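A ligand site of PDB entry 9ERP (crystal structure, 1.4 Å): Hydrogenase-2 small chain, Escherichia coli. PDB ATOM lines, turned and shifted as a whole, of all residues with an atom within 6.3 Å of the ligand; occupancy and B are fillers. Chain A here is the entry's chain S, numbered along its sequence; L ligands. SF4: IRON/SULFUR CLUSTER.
An iron atom (FE3) of the ligand is bound by a ring nitrogen (ND1) of His 191 (2.0 Å).
The side-chain sulfur (SG) of Cys 194 binds an iron atom (FE4) of the ligand (2.2 Å).
SG of Cys 225 binds FE2 of the ligand (2.3 Å).
An iron atom (FE1) of the ligand is bound by the side-chain sulfur (SG) of Cys 219 (2.3 Å).
N of Arg 197 sits close to S2 of the ligand, 3.5 Å away.
S3 of the ligand sits close to N of Leu 220 (3.6 Å).
The backbone NH of His 191 sits at hydrogen-bond distance from the backbone carbonyl oxygen of Gly 227, at 3.1 Å.
The backbone NH (N) of Arg 196 lies close to the side-chain sulfur (SG) of Cys 194 (3.4 Å).
The backbone carbonyl oxygen (O) of Leu 220 is in hydrogen-bond range of the backbone NH (N) of Cys 225 (3.3 Å).
The side-chain sulfur (SG) of Cys 225 sits close to the backbone NH (N) of Gly 227 (3.5 Å).
The side-chain sulfur of Cys 225 lies close to the backbone NH of Cys 254.
OE2 of Glu 192 lies within salt-bridge range of NH1 of Arg 197, at 3.0 Å.
The guanidinium group of Arg 196 lies within hydrogen-bond range of the backbone carbonyl oxygen of Val 248 (3.2 Å).
NH1 of Arg 196 lies within hydrogen-bond range of O of Trp 218 (2.9 Å).
O of Arg 196 sits close to S2 of the ligand (3.7 Å).
Merely in contact with the ligand: Phe 200, Tyr 221, Gly 227, Pro 228 and Val 248.
Hydrophobic or aromatic side chains within 4 Å of the ligand: His 191, Phe 200, Tyr 221, Pro 228 and Val 248.
Of the 23 residues printed, 12 come within 4 Å of the ligand.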
ATOM      1  N   ILE A 190       8.177   0.046  29.525  1.00  0.00           N
ATOM      2  CA  ILE A 190       6.897   0.276  28.841  1.00  0.00           C
ATOM      3  C   ILE A 190       7.130   0.885  27.466  1.00  0.00           C
ATOM      4  O   ILE A 190       6.513   0.473  26.480  1.00  0.00           O
ATOM      5  CB  ILE A 190       5.963   1.139  29.745  1.00  0.00           C
ATOM      6  CG1 ILE A 190       5.527   0.302  30.951  1.00  0.00           C
ATOM      7  CG2 ILE A 190       4.771   1.656  28.967  1.00  0.00           C
ATOM      8  CD1 ILE A 190       4.862   1.126  32.041  1.00  0.00           C
ATOM      9  N   HIS A 191       8.041   1.854  27.366  1.00  0.00           N
ATOM     10  CA  HIS A 191       8.311   2.508  26.087  1.00  0.00           C
ATOM     11  C   HIS A 191       8.928   1.555  25.059  1.00  0.00           C
ATOM     12  O   HIS A 191       8.871   1.859  23.858  1.00  0.00           O
ATOM     13  CB  HIS A 191       9.273   3.649  26.399  1.00  0.00           C
ATOM     14  CG  HIS A 191       9.679   4.502  25.235  1.00  0.00           C
ATOM     15  ND1 HIS A 191       8.839   5.426  24.648  1.00  0.00           N
ATOM     16  CD2 HIS A 191      10.864   4.594  24.585  1.00  0.00           C
ATOM     17  CE1 HIS A 191       9.506   6.064  23.693  1.00  0.00           C
ATOM     18  NE2 HIS A 191      10.728   5.573  23.630  1.00  0.00           N
ATOM     19  N   GLU A 192       9.556   0.460  25.475  1.00  0.00           N
ATOM     20  CA  GLU A 192      10.091  -0.530  24.552  1.00  0.00           C
ATOM     21  C   GLU A 192       9.051  -1.577  24.155  1.00  0.00           C
ATOM     22  O   GLU A 192       9.382  -2.561  23.501  1.00  0.00           O
ATOM     23  CB  GLU A 192      11.344  -1.156  25.138  1.00  0.00           C
ATOM     24  CG  GLU A 192      12.513  -0.149  25.248  1.00  0.00           C
ATOM     25  CD  GLU A 192      12.836   0.489  23.924  1.00  0.00           C
ATOM     26  OE1 GLU A 192      13.074  -0.256  22.959  1.00  0.00           O
ATOM     27  OE2 GLU A 192      12.869   1.752  23.812  1.00  0.00           O
ATOM     28  N   CYS A 194       5.429  -0.165  23.626  1.00  0.00           N
ATOM     29  CA  CYS A 194       4.270   0.726  23.637  1.00  0.00           C
ATOM     30  C   CYS A 194       3.752   0.960  22.226  1.00  0.00           C
ATOM     31  O   CYS A 194       4.538   1.274  21.306  1.00  0.00           O
ATOM     32  CB  CYS A 194       4.640   2.076  24.252  1.00  0.00           C
ATOM     33  SG  CYS A 194       3.270   3.264  24.232  1.00  0.00           S
ATOM     34  N   GLU A 195       2.437   0.849  22.057  1.00  0.00           N
ATOM     35  CA  GLU A 195       1.820   0.975  20.728  1.00  0.00           C
ATOM     36  C   GLU A 195       1.835   2.388  20.179  1.00  0.00           C
ATOM     37  O   GLU A 195       1.503   2.588  18.997  1.00  0.00           O
ATOM     38  CB  GLU A 195       0.387   0.414  20.770  1.00  0.00           C
ATOM     39  CG  GLU A 195      -0.646   1.244  21.560  1.00  0.00           C
ATOM     40  CD  GLU A 195      -0.719   0.975  23.072  1.00  0.00           C
ATOM     41  OE1 GLU A 195       0.206   0.369  23.663  1.00  0.00           O
ATOM     42  OE2 GLU A 195      -1.752   1.379  23.694  1.00  0.00           O
ATOM     43  N   ARG A 196       2.231   3.378  21.002  1.00  0.00           N
ATOM     44  CA  ARG A 196       2.361   4.736  20.504  1.00  0.00           C
ATOM     45  C   ARG A 196       3.779   5.048  20.088  1.00  0.00           C
ATOM     46  O   ARG A 196       4.058   6.182  19.666  1.00  0.00           O
ATOM     47  CB  ARG A 196       1.840   5.733  21.533  1.00  0.00           C
ATOM     48  CG  ARG A 196       0.373   5.449  21.867  1.00  0.00           C
ATOM     49  CD  ARG A 196      -0.343   6.593  22.530  1.00  0.00           C
ATOM     50  NE  ARG A 196      -1.741   6.219  22.751  1.00  0.00           N
ATOM     51  CZ  ARG A 196      -2.708   7.073  23.004  1.00  0.00           C
ATOM     52  NH1 ARG A 196      -2.459   8.365  23.167  1.00  0.00           N
ATOM     53  NH2 ARG A 196      -3.952   6.627  23.134  1.00  0.00           N
ATOM     54  N   ARG A 197       4.676   4.069  20.152  1.00  0.00           N
ATOM     55  CA  ARG A 197       6.053   4.333  19.718  1.00  0.00           C
ATOM     56  C   ARG A 197       6.131   4.838  18.290  1.00  0.00           C
ATOM     57  O   ARG A 197       6.994   5.692  18.026  1.00  0.00           O
ATOM     58  CB  ARG A 197       6.876   3.059  19.899  1.00  0.00           C
ATOM     59  CG  ARG A 197       8.336   3.202  19.462  1.00  0.00           C
ATOM     60  CD  ARG A 197       9.099   4.244  20.296  1.00  0.00           C
ATOM     61  NE  ARG A 197      10.516   4.205  19.944  1.00  0.00           N
ATOM     62  CZ  ARG A 197      11.416   3.426  20.526  1.00  0.00           C
ATOM     63  NH1 ARG A 197      11.133   2.723  21.608  1.00  0.00           N
ATOM     64  NH2 ARG A 197      12.635   3.320  19.978  1.00  0.00           N
ATOM     65  N   PRO A 198       5.317   4.381  17.330  1.00  0.00           N
ATOM     66  CA  PRO A 198       5.410   4.974  15.982  1.00  0.00           C
ATOM     67  C   PRO A 198       5.222   6.488  15.992  1.00  0.00           C
ATOM     68  O   PRO A 198       5.869   7.197  15.217  1.00  0.00           O
ATOM     69  CB  PRO A 198       4.294   4.294  15.196  1.00  0.00           C
ATOM     70  CG  PRO A 198       4.070   2.979  15.919  1.00  0.00           C
ATOM     71  CD  PRO A 198       4.289   3.323  17.376  1.00  0.00           C
ATOM     72  N   PHE A 200       5.830   8.607  18.614  1.00  0.00           N
ATOM     73  CA  PHE A 200       7.088   9.096  19.166  1.00  0.00           C
ATOM     74  C   PHE A 200       8.143   9.190  18.072  1.00  0.00           C
ATOM     75  O   PHE A 200       8.819  10.224  17.911  1.00  0.00           O
ATOM     76  CB  PHE A 200       7.545   8.129  20.266  1.00  0.00           C
ATOM     77  CG  PHE A 200       8.817   8.517  20.948  1.00  0.00           C
ATOM     78  CD1 PHE A 200       8.799   9.308  22.070  1.00  0.00           C
ATOM     79  CD2 PHE A 200      10.033   8.095  20.450  1.00  0.00           C
ATOM     80  CE1 PHE A 200      10.002   9.660  22.712  1.00  0.00           C
ATOM     81  CE2 PHE A 200      11.213   8.446  21.063  1.00  0.00           C
ATOM     82  CZ  PHE A 200      11.208   9.224  22.199  1.00  0.00           C
ATOM     83  N   PHE A 205       3.079  14.195  18.590  1.00  0.00           N
ATOM     84  CA  PHE A 205       2.942  14.312  20.021  1.00  0.00           C
ATOM     85  C   PHE A 205       1.720  15.127  20.405  1.00  0.00           C
ATOM     86  O   PHE A 205       1.466  16.181  19.820  1.00  0.00           O
ATOM     87  CB  PHE A 205       4.148  15.042  20.641  1.00  0.00           C
ATOM     88  CG  PHE A 205       5.470  14.335  20.482  1.00  0.00           C
ATOM     89  CD1 PHE A 205       5.735  13.149  21.145  1.00  0.00           C
ATOM     90  CD2 PHE A 205       6.492  14.896  19.718  1.00  0.00           C
ATOM     91  CE1 PHE A 205       6.968  12.520  21.030  1.00  0.00           C
ATOM     92  CE2 PHE A 205       7.722  14.284  19.619  1.00  0.00           C
ATOM     93  CZ  PHE A 205       7.967  13.085  20.246  1.00  0.00           C
ATOM     94  N   TRP A 218      -2.001  10.201  19.678  1.00  0.00           N
ATOM     95  CA  TRP A 218      -0.572  10.314  19.489  1.00  0.00           C
ATOM     96  C   TRP A 218       0.202  10.087  20.784  1.00  0.00           C
ATOM     97  O   TRP A 218      -0.358   9.903  21.879  1.00  0.00           O
ATOM     98  CB  TRP A 218      -0.247  11.690  18.923  1.00  0.00           C
ATOM     99  CG  TRP A 218      -0.609  11.846  17.479  1.00  0.00           C
ATOM    100  CD1 TRP A 218      -1.199  10.923  16.666  1.00  0.00           C
ATOM    101  CD2 TRP A 218      -0.425  13.020  16.690  1.00  0.00           C
ATOM    102  NE1 TRP A 218      -1.385  11.448  15.410  1.00  0.00           N
ATOM    103  CE2 TRP A 218      -0.919  12.740  15.410  1.00  0.00           C
ATOM    104  CE3 TRP A 218       0.117  14.275  16.948  1.00  0.00           C
ATOM    105  CZ2 TRP A 218      -0.872  13.682  14.368  1.00  0.00           C
ATOM    106  CZ3 TRP A 218       0.164  15.217  15.907  1.00  0.00           C
ATOM    107  CH2 TRP A 218      -0.349  14.906  14.654  1.00  0.00           C
ATOM    108  N   CYS A 219       1.535  10.076  20.663  1.00  0.00           N
ATOM    109  CA  CYS A 219       2.397   9.786  21.808  1.00  0.00           C
ATOM    110  C   CYS A 219       2.258  10.864  22.867  1.00  0.00           C
ATOM    111  O   CYS A 219       2.060  12.041  22.572  1.00  0.00           O
ATOM    112  CB  CYS A 219       3.849   9.671  21.340  1.00  0.00           C
ATOM    113  SG  CYS A 219       5.132   9.650  22.615  1.00  0.00           S
ATOM    114  N   LEU A 220       2.371  10.440  24.122  1.00  0.00           N
ATOM    115  CA  LEU A 220       2.176  11.306  25.281  1.00  0.00           C
ATOM    116  C   LEU A 220       3.487  11.752  25.932  1.00  0.00           C
ATOM    117  O   LEU A 220       3.463  12.284  27.057  1.00  0.00           O
ATOM    118  CB  LEU A 220       1.250  10.630  26.301  1.00  0.00           C
ATOM    119  CG  LEU A 220      -0.080  10.144  25.725  1.00  0.00           C
ATOM    120  CD1 LEU A 220      -0.962   9.575  26.857  1.00  0.00           C
ATOM    121  CD2 LEU A 220      -0.825  11.211  24.974  1.00  0.00           C
ATOM    122  N   TYR A 221       4.619  11.578  25.251  1.00  0.00           N
ATOM    123  CA  TYR A 221       5.918  11.918  25.840  1.00  0.00           C
ATOM    124  C   TYR A 221       5.934  13.354  26.370  1.00  0.00           C
ATOM    125  O   TYR A 221       6.386  13.615  27.489  1.00  0.00           O
ATOM    126  CB  TYR A 221       7.035  11.756  24.803  1.00  0.00           C
ATOM    127  CG  TYR A 221       8.370  12.160  25.392  1.00  0.00           C
ATOM    128  CD1 TYR A 221       9.006  11.351  26.311  1.00  0.00           C
ATOM    129  CD2 TYR A 221       8.926  13.398  25.106  1.00  0.00           C
ATOM    130  CE1 TYR A 221      10.207  11.737  26.905  1.00  0.00           C
ATOM    131  CE2 TYR A 221      10.107  13.795  25.698  1.00  0.00           C
ATOM    132  CZ  TYR A 221      10.739  12.974  26.590  1.00  0.00           C
ATOM    133  OH  TYR A 221      11.913  13.369  27.194  1.00  0.00           O
ATOM    134  N   HIS A 222       5.469  14.287  25.571  1.00  0.00           N
ATOM    135  CA  HIS A 222       5.551  15.696  25.949  1.00  0.00           C
ATOM    136  C   HIS A 222       4.490  16.124  26.938  1.00  0.00           C
ATOM    137  O   HIS A 222       4.528  17.282  27.388  1.00  0.00           O
ATOM    138  CB  HIS A 222       5.560  16.547  24.677  1.00  0.00           C
ATOM    139  CG  HIS A 222       6.917  16.593  24.055  1.00  0.00           C
ATOM    140  ND1 HIS A 222       7.983  17.260  24.635  1.00  0.00           N
ATOM    141  CD2 HIS A 222       7.403  15.981  22.953  1.00  0.00           C
ATOM    142  CE1 HIS A 222       9.059  17.075  23.890  1.00  0.00           C
ATOM    143  NE2 HIS A 222       8.740  16.314  22.858  1.00  0.00           N
ATOM    144  N   CYS A 225       4.922  11.505  29.867  1.00  0.00           N
ATOM    145  CA  CYS A 225       4.913  10.064  29.932  1.00  0.00           C
ATOM    146  C   CYS A 225       6.241   9.495  30.449  1.00  0.00           C
ATOM    147  O   CYS A 225       7.318   9.796  29.932  1.00  0.00           O
ATOM    148  CB  CYS A 225       4.594   9.481  28.548  1.00  0.00           C
ATOM    149  SG  CYS A 225       4.358   7.695  28.641  1.00  0.00           S
ATOM    150  N   LYS A 226       6.154   8.645  31.467  1.00  0.00           N
ATOM    151  CA  LYS A 226       7.320   8.040  32.078  1.00  0.00           C
ATOM    152  C   LYS A 226       7.617   6.645  31.529  1.00  0.00           C
ATOM    153  O   LYS A 226       8.525   5.954  32.016  1.00  0.00           O
ATOM    154  CB  LYS A 226       7.207   8.014  33.600  1.00  0.00           C
ATOM    155  CG  LYS A 226       6.981   9.384  34.227  1.00  0.00           C
ATOM    156  CD  LYS A 226       8.006  10.420  33.773  1.00  0.00           C
ATOM    157  CE  LYS A 226       7.891  11.695  34.600  1.00  0.00           C
ATOM    158  NZ  LYS A 226       6.525  12.291  34.517  1.00  0.00           N
ATOM    159  N   GLY A 227       6.891   6.213  30.491  1.00  0.00           N
ATOM    160  CA  GLY A 227       7.183   4.942  29.867  1.00  0.00           C
ATOM    161  C   GLY A 227       8.640   4.717  29.557  1.00  0.00           C
ATOM    162  O   GLY A 227       9.133   3.595  29.719  1.00  0.00           O
ATOM    163  N   PRO A 228       9.374   5.743  29.127  1.00  0.00           N
ATOM    164  CA  PRO A 228      10.804   5.528  28.794  1.00  0.00           C
ATOM    165  C   PRO A 228      11.683   5.116  29.957  1.00  0.00           C
ATOM    166  O   PRO A 228      12.812   4.667  29.725  1.00  0.00           O
ATOM    167  CB  PRO A 228      11.248   6.861  28.186  1.00  0.00           C
ATOM    168  CG  PRO A 228       9.990   7.462  27.612  1.00  0.00           C
ATOM    169  CD  PRO A 228       8.896   7.044  28.622  1.00  0.00           C
ATOM    170  N   TRP A 246      -5.329   0.940  29.611  1.00  0.00           N
ATOM    171  CA  TRP A 246      -4.220   1.344  30.463  1.00  0.00           C
ATOM    172  C   TRP A 246      -4.117   2.849  30.390  1.00  0.00           C
ATOM    173  O   TRP A 246      -4.807   3.487  29.576  1.00  0.00           O
ATOM    174  CB  TRP A 246      -2.917   0.634  30.066  1.00  0.00           C
ATOM    175  CG  TRP A 246      -2.227   0.989  28.780  1.00  0.00           C
ATOM    176  CD1 TRP A 246      -2.643   0.702  27.502  1.00  0.00           C
ATOM    177  CD2 TRP A 246      -0.922   1.582  28.654  1.00  0.00           C
ATOM    178  NE1 TRP A 246      -1.698   1.110  26.596  1.00  0.00           N
ATOM    179  CE2 TRP A 246      -0.630   1.631  27.272  1.00  0.00           C
ATOM    180  CE3 TRP A 246       0.035   2.039  29.571  1.00  0.00           C
ATOM    181  CZ2 TRP A 246       0.574   2.173  26.786  1.00  0.00           C
ATOM    182  CZ3 TRP A 246       1.234   2.552  29.088  1.00  0.00           C
ATOM    183  CH2 TRP A 246       1.483   2.610  27.708  1.00  0.00           C
ATOM    184  N   VAL A 248      -2.139   5.242  29.255  1.00  0.00           N
ATOM    185  CA  VAL A 248      -1.815   5.903  27.999  1.00  0.00           C
ATOM    186  C   VAL A 248      -2.931   5.699  26.995  1.00  0.00           C
ATOM    187  O   VAL A 248      -3.334   6.631  26.286  1.00  0.00           O
ATOM    188  CB  VAL A 248      -0.460   5.389  27.499  1.00  0.00           C
ATOM    189  CG1 VAL A 248      -0.286   5.718  26.023  1.00  0.00           C
ATOM    190  CG2 VAL A 248       0.676   5.984  28.330  1.00  0.00           C
ATOM    191  N   PRO A 253      -0.504  10.286  30.374  1.00  0.00           N
ATOM    192  CA  PRO A 253       0.851   9.706  30.452  1.00  0.00           C
ATOM    193  C   PRO A 253       1.018   8.724  31.601  1.00  0.00           C
ATOM    194  O   PRO A 253       0.348   8.812  32.638  1.00  0.00           O
ATOM    195  CB  PRO A 253       1.741  10.939  30.658  1.00  0.00           C
ATOM    196  CG  PRO A 253       0.803  11.987  31.208  1.00  0.00           C
ATOM    197  CD  PRO A 253      -0.488  11.745  30.509  1.00  0.00           C
ATOM    198  N   CYS A 254       1.902   7.748  31.391  1.00  0.00           N
ATOM    199  CA  CYS A 254       2.440   6.984  32.502  1.00  0.00           C
ATOM    200  C   CYS A 254       3.125   7.938  33.474  1.00  0.00           C
ATOM    201  O   CYS A 254       3.819   8.879  33.065  1.00  0.00           O
ATOM    202  CB  CYS A 254       3.454   5.940  31.994  1.00  0.00           C
ATOM    203  SG  CYS A 254       4.329   4.988  33.270  1.00  0.00           S
HETATM  204 FE1  SF4 L   1       5.074   7.727  23.875  1.00  0.00          FE
HETATM  205 FE2  SF4 L   1       4.910   7.009  26.551  1.00  0.00          FE
HETATM  206 FE3  SF4 L   1       6.928   6.022  24.984  1.00  0.00          FE
HETATM  207 FE4  SF4 L   1       4.358   5.199  24.589  1.00  0.00          FE
HETATM  208  S1  SF4 L   1       5.688   4.895  26.486  1.00  0.00           S
HETATM  209  S2  SF4 L   1       5.811   5.781  22.940  1.00  0.00           S
HETATM  210  S3  SF4 L   1       3.214   7.096  24.987  1.00  0.00           S
HETATM  211  S4  SF4 L   1       6.597   8.204  25.592  1.00  0.00           S
